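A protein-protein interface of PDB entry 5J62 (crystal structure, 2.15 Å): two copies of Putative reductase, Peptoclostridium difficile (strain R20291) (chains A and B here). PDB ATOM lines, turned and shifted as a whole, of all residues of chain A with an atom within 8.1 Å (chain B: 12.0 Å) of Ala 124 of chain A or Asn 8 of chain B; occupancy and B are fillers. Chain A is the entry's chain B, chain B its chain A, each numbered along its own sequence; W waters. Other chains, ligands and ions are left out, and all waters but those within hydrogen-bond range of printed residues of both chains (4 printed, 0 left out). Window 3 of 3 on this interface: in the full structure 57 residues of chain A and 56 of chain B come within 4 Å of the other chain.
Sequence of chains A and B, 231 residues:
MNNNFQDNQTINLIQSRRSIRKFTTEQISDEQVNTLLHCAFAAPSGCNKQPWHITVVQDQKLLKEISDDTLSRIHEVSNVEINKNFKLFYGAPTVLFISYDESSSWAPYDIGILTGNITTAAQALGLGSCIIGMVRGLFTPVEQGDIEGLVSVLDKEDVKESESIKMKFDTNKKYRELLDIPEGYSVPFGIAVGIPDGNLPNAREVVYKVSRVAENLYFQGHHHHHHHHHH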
ATOM      1  N   GLN A   9      12.050   2.602 -10.914  1.00  0.00           N
ATOM      2  CA  GLN A   9      11.614   3.924 -11.289  1.00  0.00           C
ATOM      3  C   GLN A   9      10.079   4.104 -11.136  1.00  0.00           C
ATOM      4  O   GLN A   9       9.630   5.179 -10.819  1.00  0.00           O
ATOM      5  CB  GLN A   9      12.101   4.243 -12.721  1.00  0.00           C
ATOM      6  CG  GLN A   9      11.373   5.367 -13.492  1.00  0.00           C
ATOM      7  CD  GLN A   9      11.172   5.050 -15.010  1.00  0.00           C
ATOM      8  OE1 GLN A   9      12.084   4.481 -15.645  1.00  0.00           O
ATOM      9  NE2 GLN A   9       9.973   5.415 -15.596  1.00  0.00           N
ATOM     10  N   THR A  10       9.285   3.089 -11.440  1.00  0.00           N
ATOM     11  CA  THR A  10       7.852   3.218 -11.387  1.00  0.00           C
ATOM     12  C   THR A  10       7.395   3.386  -9.875  1.00  0.00           C
ATOM     13  O   THR A  10       6.576   4.215  -9.562  1.00  0.00           O
ATOM     14  CB  THR A  10       7.165   1.999 -12.021  1.00  0.00           C
ATOM     15  OG1 THR A  10       7.476   1.958 -13.428  1.00  0.00           O
ATOM     16  CG2 THR A  10       5.600   2.104 -11.865  1.00  0.00           C
ATOM     17  N   LEU A  13       8.326   6.948  -8.673  1.00  0.00           N
ATOM     18  CA  LEU A  13       7.336   7.888  -9.156  1.00  0.00           C
ATOM     19  C   LEU A  13       6.006   7.887  -8.391  1.00  0.00           C
ATOM     20  O   LEU A  13       5.496   8.938  -8.072  1.00  0.00           O
ATOM     21  CB  LEU A  13       7.028   7.711 -10.621  1.00  0.00           C
ATOM     22  CG  LEU A  13       8.118   8.109 -11.623  1.00  0.00           C
ATOM     23  CD1 LEU A  13       7.605   7.736 -12.997  1.00  0.00           C
ATOM     24  CD2 LEU A  13       8.530   9.570 -11.620  1.00  0.00           C
ATOM     25  N   GLN A  32       2.460  13.133 -26.374  1.00  0.00           N
ATOM     26  CA  GLN A  32       2.233  13.103 -24.938  1.00  0.00           C
ATOM     27  C   GLN A  32       0.748  12.977 -24.678  1.00  0.00           C
ATOM     28  O   GLN A  32       0.321  12.066 -23.968  1.00  0.00           O
ATOM     29  CB  GLN A  32       2.853  14.301 -24.234  1.00  0.00           C
ATOM     30  CG  GLN A  32       4.365  14.183 -24.242  1.00  0.00           C
ATOM     31  CD  GLN A  32       5.053  15.471 -23.720  1.00  0.00           C
ATOM     32  OE1 GLN A  32       4.593  16.591 -23.947  1.00  0.00           O
ATOM     33  NE2 GLN A  32       6.152  15.284 -23.001  1.00  0.00           N
ATOM     34  N   THR A  35      -0.254   9.435 -25.523  1.00  0.00           N
ATOM     35  CA  THR A  35       0.210   8.480 -24.515  1.00  0.00           C
ATOM     36  C   THR A  35      -0.688   8.529 -23.219  1.00  0.00           C
ATOM     37  O   THR A  35      -1.119   7.506 -22.682  1.00  0.00           O
ATOM     38  CB  THR A  35       1.720   8.682 -24.229  1.00  0.00           C
ATOM     39  OG1 THR A  35       2.468   8.312 -25.390  1.00  0.00           O
ATOM     40  CG2 THR A  35       2.192   7.782 -23.131  1.00  0.00           C
ATOM     41  N   LEU A  36      -0.977   9.715 -22.760  1.00  0.00           N
ATOM     42  CA  LEU A  36      -1.881   9.917 -21.603  1.00  0.00           C
ATOM     43  C   LEU A  36      -3.226   9.227 -21.827  1.00  0.00           C
ATOM     44  O   LEU A  36      -3.707   8.483 -20.978  1.00  0.00           O
ATOM     45  CB  LEU A  36      -2.067  11.403 -21.303  1.00  0.00           C
ATOM     46  CG  LEU A  36      -0.868  12.201 -20.802  1.00  0.00           C
ATOM     47  CD1 LEU A  36      -1.184  13.688 -20.701  1.00  0.00           C
ATOM     48  CD2 LEU A  36      -0.398  11.671 -19.463  1.00  0.00           C
ATOM     49  N   CYS A  39      -2.846   5.317 -21.895  1.00  0.00           N
ATOM     50  CA  CYS A  39      -2.770   4.899 -20.487  1.00  0.00           C
ATOM     51  C   CYS A  39      -4.128   4.957 -19.771  1.00  0.00           C
ATOM     52  O   CYS A  39      -4.534   4.011 -19.120  1.00  0.00           O
ATOM     53  CB  CYS A  39      -1.740   5.758 -19.742  1.00  0.00           C
ATOM     54  SG  CYS A  39      -0.027   5.405 -20.310  1.00  0.00           S
ATOM     55  N   ASN A 117      -4.052   6.365 -13.687  1.00  0.00           N
ATOM     56  CA  ASN A 117      -3.210   5.973 -14.781  1.00  0.00           C
ATOM     57  C   ASN A 117      -2.721   7.254 -15.467  1.00  0.00           C
ATOM     58  O   ASN A 117      -1.542   7.402 -15.765  1.00  0.00           O
ATOM     59  CB  ASN A 117      -3.998   5.142 -15.834  1.00  0.00           C
ATOM     60  CG  ASN A 117      -4.088   3.689 -15.478  1.00  0.00           C
ATOM     61  OD1 ASN A 117      -3.641   3.280 -14.451  1.00  0.00           O
ATOM     62  ND2 ASN A 117      -4.638   2.876 -16.377  1.00  0.00           N
ATOM     63  N   ILE A 118      -3.619   8.194 -15.688  1.00  0.00           N
ATOM     64  CA  ILE A 118      -3.212   9.465 -16.301  1.00  0.00           C
ATOM     65  C   ILE A 118      -2.176  10.229 -15.467  1.00  0.00           C
ATOM     66  O   ILE A 118      -1.218  10.773 -15.988  1.00  0.00           O
ATOM     67  CB  ILE A 118      -4.416  10.386 -16.467  1.00  0.00           C
ATOM     68  CG1 ILE A 118      -5.312   9.834 -17.549  1.00  0.00           C
ATOM     69  CG2 ILE A 118      -4.012  11.817 -16.847  1.00  0.00           C
ATOM     70  CD1 ILE A 118      -6.625  10.577 -17.695  1.00  0.00           C
ATOM     71  N   THR A 119      -2.444  10.307 -14.169  1.00  0.00           N
ATOM     72  CA  THR A 119      -1.607  10.972 -13.186  1.00  0.00           C
ATOM     73  C   THR A 119      -0.186  10.390 -13.207  1.00  0.00           C
ATOM     74  O   THR A 119       0.788  11.130 -13.278  1.00  0.00           O
ATOM     75  CB  THR A 119      -2.262  10.793 -11.775  1.00  0.00           C
ATOM     76  OG1 THR A 119      -3.465  11.590 -11.721  1.00  0.00           O
ATOM     77  CG2 THR A 119      -1.389  11.222 -10.714  1.00  0.00           C
ATOM     78  N   THR A 120      -0.081   9.071 -13.105  1.00  0.00           N
ATOM     79  CA  THR A 120       1.209   8.411 -13.118  1.00  0.00           C
ATOM     80  C   THR A 120       1.874   8.534 -14.487  1.00  0.00           C
ATOM     81  O   THR A 120       3.094   8.788 -14.582  1.00  0.00           O
ATOM     82  CB  THR A 120       1.044   6.946 -12.657  1.00  0.00           C
ATOM     83  OG1 THR A 120       0.501   6.964 -11.343  1.00  0.00           O
ATOM     84  CG2 THR A 120       2.353   6.248 -12.620  1.00  0.00           C
ATOM     85  N   ALA A 121       1.090   8.391 -15.552  1.00  0.00           N
ATOM     86  CA  ALA A 121       1.691   8.493 -16.884  1.00  0.00           C
ATOM     87  C   ALA A 121       2.269   9.860 -17.072  1.00  0.00           C
ATOM     88  O   ALA A 121       3.407   9.967 -17.555  1.00  0.00           O
ATOM     89  CB  ALA A 121       0.692   8.131 -17.979  1.00  0.00           C
ATOM     90  N   ALA A 122       1.575  10.908 -16.588  1.00  0.00           N
ATOM     91  CA  ALA A 122       2.095  12.271 -16.698  1.00  0.00           C
ATOM     92  C   ALA A 122       3.445  12.426 -16.026  1.00  0.00           C
ATOM     93  O   ALA A 122       4.350  12.985 -16.609  1.00  0.00           O
ATOM     94  CB  ALA A 122       1.127  13.322 -16.170  1.00  0.00           C
ATOM     95  N   GLN A 123       3.588  11.909 -14.817  1.00  0.00           N
ATOM     96  CA  GLN A 123       4.878  11.910 -14.168  1.00  0.00           C
ATOM     97  C   GLN A 123       5.929  11.237 -15.030  1.00  0.00           C
ATOM     98  O   GLN A 123       7.090  11.695 -15.092  1.00  0.00           O
ATOM     99  CB  GLN A 123       4.848  11.147 -12.866  1.00  0.00           C
ATOM    100  CG  GLN A 123       4.028  11.779 -11.700  1.00  0.00           C
ATOM    101  CD  GLN A 123       4.062  10.855 -10.479  1.00  0.00           C
ATOM    102  OE1 GLN A 123       3.178   9.984 -10.324  1.00  0.00           O
ATOM    103  NE2 GLN A 123       5.126  10.955  -9.675  1.00  0.00           N
ATOM    104  N   ALA A 124       5.559  10.099 -15.617  1.00  0.00           N
ATOM    105  CA  ALA A 124       6.517   9.288 -16.327  1.00  0.00           C
ATOM    106  C   ALA A 124       7.076  10.011 -17.536  1.00  0.00           C
ATOM    107  O   ALA A 124       8.176   9.729 -17.914  1.00  0.00           O
ATOM    108  CB  ALA A 124       5.928   7.942 -16.763  1.00  0.00           C
ATOM    109  N   LEU A 125       6.278  10.895 -18.123  1.00  0.00           N
ATOM    110  CA  LEU A 125       6.610  11.692 -19.286  1.00  0.00           C
ATOM    111  C   LEU A 125       7.336  12.996 -18.977  1.00  0.00           C
ATOM    112  O   LEU A 125       7.517  13.793 -19.868  1.00  0.00           O
ATOM    113  CB  LEU A 125       5.292  12.053 -20.046  1.00  0.00           C
ATOM    114  CG  LEU A 125       4.545  10.855 -20.659  1.00  0.00           C
ATOM    115  CD1 LEU A 125       3.191  11.294 -21.183  1.00  0.00           C
ATOM    116  CD2 LEU A 125       5.390  10.240 -21.770  1.00  0.00           C
ATOM    117  N   GLY A 126       7.705  13.249 -17.733  1.00  0.00           N
ATOM    118  CA  GLY A 126       8.324  14.516 -17.378  1.00  0.00           C
ATOM    119  C   GLY A 126       7.315  15.604 -17.164  1.00  0.00           C
ATOM    120  O   GLY A 126       7.670  16.785 -17.155  1.00  0.00           O
ATOM    121  N   LEU A 127       6.040  15.227 -16.973  1.00  0.00           N
ATOM    122  CA  LEU A 127       4.995  16.186 -16.769  1.00  0.00           C
ATOM    123  C   LEU A 127       4.519  16.191 -15.295  1.00  0.00           C
ATOM    124  O   LEU A 127       5.140  15.572 -14.422  1.00  0.00           O
ATOM    125  CB  LEU A 127       3.867  15.963 -17.771  1.00  0.00           C
ATOM    126  CG  LEU A 127       4.186  16.001 -19.267  1.00  0.00           C
ATOM    127  CD1 LEU A 127       2.955  15.638 -20.052  1.00  0.00           C
ATOM    128  CD2 LEU A 127       4.690  17.399 -19.734  1.00  0.00           C
ATOM    129  N   GLY A 128       3.442  16.939 -15.040  1.00  0.00           N
ATOM    130  CA  GLY A 128       2.811  17.043 -13.773  1.00  0.00           C
ATOM    131  C   GLY A 128       1.362  17.370 -13.991  1.00  0.00           C
ATOM    132  O   GLY A 128       0.996  17.746 -15.090  1.00  0.00           O
ATOM    133  N   GLN B   6       5.940   3.231 -25.261  1.00  0.00           N
ATOM    134  CA  GLN B   6       7.321   3.752 -25.471  1.00  0.00           C
ATOM    135  C   GLN B   6       8.335   2.771 -24.808  1.00  0.00           C
ATOM    136  O   GLN B   6       7.917   1.720 -24.278  1.00  0.00           O
ATOM    137  CB  GLN B   6       7.403   5.199 -24.906  1.00  0.00           C
ATOM    138  CG  GLN B   6       6.348   6.175 -25.468  1.00  0.00           C
ATOM    139  CD  GLN B   6       6.449   7.581 -24.879  1.00  0.00           C
ATOM    140  OE1 GLN B   6       7.411   7.902 -24.185  1.00  0.00           O
ATOM    141  NE2 GLN B   6       5.454   8.439 -25.171  1.00  0.00           N
ATOM    142  N   ASP B   7       9.619   3.144 -24.875  1.00  0.00           N
ATOM    143  CA  ASP B   7      10.722   2.529 -24.118  1.00  0.00           C
ATOM    144  C   ASP B   7      10.799   3.079 -22.662  1.00  0.00           C
ATOM    145  O   ASP B   7      11.761   2.834 -21.933  1.00  0.00           O
ATOM    146  CB  ASP B   7      12.018   2.826 -24.864  1.00  0.00           C
ATOM    147  CG  ASP B   7      12.064   4.243 -25.345  1.00  0.00           C
ATOM    148  OD1 ASP B   7      11.763   5.122 -24.520  1.00  0.00           O
ATOM    149  OD2 ASP B   7      12.351   4.484 -26.528  1.00  0.00           O
ATOM    150  N   ASN B   8       9.786   3.839 -22.265  1.00  0.00           N
ATOM    151  CA  ASN B   8       9.572   4.227 -20.895  1.00  0.00           C
ATOM    152  C   ASN B   8       8.847   3.062 -20.192  1.00  0.00           C
ATOM    153  O   ASN B   8       7.706   2.654 -20.541  1.00  0.00           O
ATOM    154  CB  ASN B   8       8.730   5.472 -20.891  1.00  0.00           C
ATOM    155  CG  ASN B   8       8.551   6.046 -19.510  1.00  0.00           C
ATOM    156  OD1 ASN B   8       8.023   5.383 -18.581  1.00  0.00           O
ATOM    157  ND2 ASN B   8       8.932   7.290 -19.367  1.00  0.00           N
ATOM    158  N   GLN B   9       9.525   2.548 -19.188  1.00  0.00           N
ATOM    159  CA  GLN B   9       9.125   1.336 -18.465  1.00  0.00           C
ATOM    160  C   GLN B   9       7.741   1.534 -17.774  1.00  0.00           C
ATOM    161  O   GLN B   9       6.886   0.682 -17.843  1.00  0.00           O
ATOM    162  CB  GLN B   9      10.187   1.107 -17.425  1.00  0.00           C
ATOM    163  CG  GLN B   9      10.479  -0.303 -16.995  1.00  0.00           C
ATOM    164  CD  GLN B   9      11.873  -0.377 -16.307  1.00  0.00           C
ATOM    165  OE1 GLN B   9      12.748  -1.144 -16.748  1.00  0.00           O
ATOM    166  NE2 GLN B   9      12.087   0.455 -15.239  1.00  0.00           N
ATOM    167  N   THR B  10       7.525   2.690 -17.161  1.00  0.00           N
ATOM    168  CA  THR B  10       6.260   3.013 -16.502  1.00  0.00           C
ATOM    169  C   THR B  10       5.089   3.045 -17.494  1.00  0.00           C
ATOM    170  O   THR B  10       4.046   2.427 -17.251  1.00  0.00           O
ATOM    171  CB  THR B  10       6.354   4.318 -15.750  1.00  0.00           C
ATOM    172  OG1 THR B  10       7.369   4.208 -14.740  1.00  0.00           O
ATOM    173  CG2 THR B  10       4.965   4.659 -15.063  1.00  0.00           C
ATOM    174  N   ILE B  11       5.273   3.739 -18.600  1.00  0.00           N
ATOM    175  CA  ILE B  11       4.256   3.789 -19.666  1.00  0.00           C
ATOM    176  C   ILE B  11       3.928   2.392 -20.194  1.00  0.00           C
ATOM    177  O   ILE B  11       2.748   1.999 -20.364  1.00  0.00           O
ATOM    178  CB  ILE B  11       4.664   4.763 -20.777  1.00  0.00           C
ATOM    179  CG1 ILE B  11       4.436   6.207 -20.289  1.00  0.00           C
ATOM    180  CG2 ILE B  11       3.793   4.537 -22.010  1.00  0.00           C
ATOM    181  CD1 ILE B  11       5.691   6.895 -20.012  1.00  0.00           C
ATOM    182  N   ASN B  12       4.955   1.590 -20.354  1.00  0.00           N
ATOM    183  CA  ASN B  12       4.727   0.259 -20.905  1.00  0.00           C
ATOM    184  C   ASN B  12       3.931  -0.592 -19.934  1.00  0.00           C
ATOM    185  O   ASN B  12       3.075  -1.323 -20.377  1.00  0.00           O
ATOM    186  CB  ASN B  12       6.066  -0.427 -21.249  1.00  0.00           C
ATOM    187  CG  ASN B  12       5.877  -1.783 -21.987  1.00  0.00           C
ATOM    188  OD1 ASN B  12       6.568  -2.792 -21.696  1.00  0.00           O
ATOM    189  ND2 ASN B  12       4.945  -1.809 -22.940  1.00  0.00           N
ATOM    190  N   LEU B  13       4.234  -0.546 -18.620  1.00  0.00           N
ATOM    191  CA  LEU B  13       3.399  -1.286 -17.654  1.00  0.00           C
ATOM    192  C   LEU B  13       1.953  -0.809 -17.720  1.00  0.00           C
ATOM    193  O   LEU B  13       1.023  -1.595 -17.830  1.00  0.00           O
ATOM    194  CB  LEU B  13       3.926  -1.168 -16.235  1.00  0.00           C
ATOM    195  CG  LEU B  13       5.268  -1.813 -16.040  1.00  0.00           C
ATOM    196  CD1 LEU B  13       5.747  -1.473 -14.640  1.00  0.00           C
ATOM    197  CD2 LEU B  13       5.212  -3.343 -16.275  1.00  0.00           C
ATOM    198  N   ILE B  14       1.738   0.510 -17.702  1.00  0.00           N
ATOM    199  CA  ILE B  14       0.368   0.975 -17.610  1.00  0.00           C
ATOM    200  C   ILE B  14      -0.429   0.538 -18.841  1.00  0.00           C
ATOM    201  O   ILE B  14      -1.566   0.096 -18.746  1.00  0.00           O
ATOM    202  CB  ILE B  14       0.316   2.481 -17.438  1.00  0.00           C
ATOM    203  CG1 ILE B  14       0.830   2.829 -16.050  1.00  0.00           C
ATOM    204  CG2 ILE B  14      -1.113   2.978 -17.566  1.00  0.00           C
ATOM    205  CD1 ILE B  14       1.123   4.273 -15.836  1.00  0.00           C
ATOM    206  N   GLN B  15       0.203   0.667 -19.997  1.00  0.00           N
ATOM    207  CA  GLN B  15      -0.449   0.302 -21.268  1.00  0.00           C
ATOM    208  C   GLN B  15      -0.620  -1.183 -21.429  1.00  0.00           C
ATOM    209  O   GLN B  15      -1.589  -1.601 -22.058  1.00  0.00           O
ATOM    210  CB  GLN B  15       0.319   0.853 -22.462  1.00  0.00           C
ATOM    211  CG  GLN B  15       0.318   2.355 -22.428  1.00  0.00           C
ATOM    212  CD  GLN B  15       0.986   2.969 -23.659  1.00  0.00           C
ATOM    213  OE1 GLN B  15       1.600   2.287 -24.465  1.00  0.00           O
ATOM    214  NE2 GLN B  15       0.841   4.236 -23.796  1.00  0.00           N
ATOM    215  N   SER B  16       0.237  -1.991 -20.814  1.00  0.00           N
ATOM    216  CA  SER B  16       0.122  -3.435 -21.020  1.00  0.00           C
ATOM    217  C   SER B  16      -0.611  -4.172 -19.909  1.00  0.00           C
ATOM    218  O   SER B  16      -0.773  -5.393 -19.971  1.00  0.00           O
ATOM    219  CB  SER B  16       1.513  -4.033 -21.290  1.00  0.00           C
ATOM    220  OG  SER B  16       2.332  -3.779 -20.187  1.00  0.00           O
ATOM    221  N   ARG B  17      -1.108  -3.435 -18.923  1.00  0.00           N
ATOM    222  CA  ARG B  17      -1.726  -4.080 -17.772  1.00  0.00           C
ATOM    223  C   ARG B  17      -2.899  -4.935 -18.182  1.00  0.00           C
ATOM    224  O   ARG B  17      -3.720  -4.500 -18.960  1.00  0.00           O
ATOM    225  CB  ARG B  17      -2.165  -3.025 -16.765  1.00  0.00           C
ATOM    226  CG  ARG B  17      -2.855  -3.547 -15.468  1.00  0.00           C
ATOM    227  CD  ARG B  17      -4.053  -2.668 -15.142  1.00  0.00           C
ATOM    228  NE  ARG B  17      -4.967  -2.541 -16.245  1.00  0.00           N
ATOM    229  CZ  ARG B  17      -5.877  -3.452 -16.582  1.00  0.00           C
ATOM    230  NH1 ARG B  17      -6.017  -4.574 -15.896  1.00  0.00           N
ATOM    231  NH2 ARG B  17      -6.653  -3.234 -17.637  1.00  0.00           N
ATOM    232  N   ASN B 117      -2.798   2.962  -8.169  1.00  0.00           N
ATOM    233  CA  ASN B 117      -1.432   2.890  -7.617  1.00  0.00           C
ATOM    234  C   ASN B 117      -1.034   1.482  -7.206  1.00  0.00           C
ATOM    235  O   ASN B 117       0.072   1.074  -7.472  1.00  0.00           O
ATOM    236  CB  ASN B 117      -1.271   3.766  -6.405  1.00  0.00           C
ATOM    237  CG  ASN B 117      -1.136   5.231  -6.745  1.00  0.00           C
ATOM    238  OD1 ASN B 117      -1.278   5.625  -7.865  1.00  0.00           O
ATOM    239  ND2 ASN B 117      -0.890   6.050  -5.722  1.00  0.00           N
ATOM    240  N   THR B 120      -0.532  -0.781 -10.606  1.00  0.00           N
ATOM    241  CA  THR B 120       0.681  -0.437 -11.280  1.00  0.00           C
ATOM    242  C   THR B 120       1.884  -0.831 -10.429  1.00  0.00           C
ATOM    243  O   THR B 120       2.795  -1.471 -10.919  1.00  0.00           O
ATOM    244  CB  THR B 120       0.664   1.057 -11.596  1.00  0.00           C
ATOM    245  OG1 THR B 120      -0.500   1.309 -12.329  1.00  0.00           O
ATOM    246  CG2 THR B 120       1.839   1.491 -12.471  1.00  0.00           C
ATOM    247  N   GLN B 123       2.504  -4.572 -10.703  1.00  0.00           N
ATOM    248  CA  GLN B 123       3.158  -4.824 -11.977  1.00  0.00           C
ATOM    249  C   GLN B 123       4.645  -4.514 -11.907  1.00  0.00           C
ATOM    250  O   GLN B 123       5.463  -5.247 -12.509  1.00  0.00           O
ATOM    251  CB  GLN B 123       2.568  -3.946 -13.089  1.00  0.00           C
ATOM    252  CG  GLN B 123       1.218  -4.396 -13.659  1.00  0.00           C
ATOM    253  CD  GLN B 123       0.746  -3.446 -14.683  1.00  0.00           C
ATOM    254  OE1 GLN B 123       0.104  -2.427 -14.344  1.00  0.00           O
ATOM    255  NE2 GLN B 123       1.052  -3.732 -15.963  1.00  0.00           N
ATOM    256  N   ALA B 124       4.999  -3.408 -11.243  1.00  0.00           N
ATOM    257  CA  ALA B 124       6.390  -2.971 -11.218  1.00  0.00           C
ATOM    258  C   ALA B 124       7.216  -3.892 -10.367  1.00  0.00           C
ATOM    259  O   ALA B 124       8.396  -3.889 -10.513  1.00  0.00           O
ATOM    260  CB  ALA B 124       6.544  -1.573 -10.685  1.00  0.00           C
HETATM  261  O   HOH W   1      -3.386   0.166 -16.576  1.00  0.00           O
HETATM  262  O   HOH W   2       9.716   0.496 -13.603  1.00  0.00           O
HETATM  263  O   HOH W   3       2.105   5.668 -25.779  1.00  0.00           O
HETATM  264  O   HOH W   4      13.679   0.969 -12.592  1.00  0.00           O
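Gln 9 of chain A touches Asn 8 of chain B (NE2 to OD1, 3.6 Å). Leu 13 of chain A touches Thr 10 of chain B (CD1 to OG1, 3.9 Å). Thr 35 of chain A touches Ile 11 of chain B (CG2 to CG2, 3.8 Å). Thr 35 of chain A touches Gln 15 of chain B (CG2 to NE2, 3.9 Å). Ile 14 of chain B touches Asn 117 of chain A (CG2 to CG, 3.7 Å). CG2 of Thr 120 of chain A touches CG2 of Thr 10 of chain B, at 3.9 Å. Ile 14 of chain B touches Thr 120 of chain A. Ala 124 of chain A touches Thr 10 of chain B. Ala 124 of chain A touches Ile 11 of chain B. Leu 125 of chain A touches Ile 11 of chain B.
The side-chain amide oxygen (OD1) of Asn 8 of chain B is in hydrogen-bond range of the backbone NH (N) of Thr 10 of chain B. The backbone NH (N) of Ile 11 of chain B lies close to the side-chain amide oxygen (OD1) of Asn 8 of chain B (3.2 Å). The side-chain amide nitrogen (NE2) of Gln 123 of chain A sits at hydrogen-bond distance from the backbone carbonyl oxygen (O) of Leu 13 of chain A, 2.6 Å away. The side-chain sulfur (SG) of Cys 39 of chain A sits at hydrogen-bond distance from the backbone carbonyl oxygen (O) of Thr 35 of chain A (3.4 Å). O of Cys 39 of chain A is in hydrogen-bond range of ND2 of Asn 117 of chain A (3.0 Å).
Water W2 lies within hydrogen-bond range of the side-chain hydroxyl (OG1) of Thr 10 of chain A (2.7 Å) and the side-chain amide nitrogen (NE2) of Gln 9 of chain B (2.9 Å). Water W3 lies within hydrogen-bond range of OG1 of Thr 35 of chain A (2.7 Å) and NE2 of Gln 15 of chain B (2.8 Å). Water W1 lies within hydrogen-bond range of O of Ile 14 of chain B, ND2 of Asn 117 of chain A and NE of Arg 17 of chain B. Water W4 bridges the backbone NH of Gln 9 of chain A and the side-chain amide nitrogen of Gln 9 of chain B.
Of the 19 printed residues of chain A, 9 touch a printed residue of chain B. Printed residues of chain A that touch a printed residue of chain B: Gln 9, Thr 10, Leu 13, Thr 35, Cys 39, Asn 117, Thr 120, Ala 124 and Leu 125. Hydrophobic or aromatic side chains of chain B that line the printed part of chain A: Ile 11, Ile 14 and Ala 124.
The side-chain amide nitrogen (NE2) of Gln 6 of chain B is in hydrogen-bond range of the side-chain hydroxyl (OG1) of Thr 35 of chain A. O of Ala 124 of chain A lies within hydrogen-bond range of ND2 of Asn 8 of chain B (2.9 Å). NE2 of Gln 9 of chain A lies within hydrogen-bond range of OG1 of Thr 10 of chain B, at 3.0 Å. The side-chain hydroxyl of Thr 10 of chain A lies within hydrogen-bond range of the side-chain hydroxyl of Thr 10 of chain B (2.6 Å). The side-chain sulfur (SG) of Cys 39 of chain A lies close to the side-chain amide nitrogen (NE2) of Gln 15 of chain B.
Gln 9 of chain A touches Thr 10 of chain B, but with the chains exchanged Thr 10 of chain A does not touch Gln 9 of chain B (4.4 Å). Thr 10 of chain B touches its own counterpart, Thr 10 of chain A. Thr 10 of chain A touches Ala 124 of chain B, and with the chains exchanged Ala 124 of chain A touches Thr 10 of chain B. Leu 13 of chain A touches Thr 10 of chain B, but with the chains exchanged Thr 10 of chain A does not touch Leu 13 of chain B (4.03 Å).
Of chain B, only Asn 8 (2.9 Å), Thr 10 (3.8 Å) and Ile 11 (3.4 Å) come within 4 Å of Ala 124 of chain A. Of the printed residues of chain B, Thr 120 of chain A touches Thr 10 and Ile 14. No residue of chain B comes within 4 Å of Ala 121 of chain A. No residue of chain B comes within 4 Å of Ala 122 of chain A. No residue of chain B comes within 4 Å of Gln 123 of chain A. No residue of chain B comes within 4 Å of Gly 126 of chain A. Of the printed residues of chain A, Thr 120 of chain B touches Thr 10. Of the printed residues of chain A, Gln 6 of chain B touches Thr 35 (3.0 Å) and Leu 125 (3.8 Å). The nearest printed residue of chain B that does not touch Asn 117 of chain A is Thr 120 of chain B (4.3 Å).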
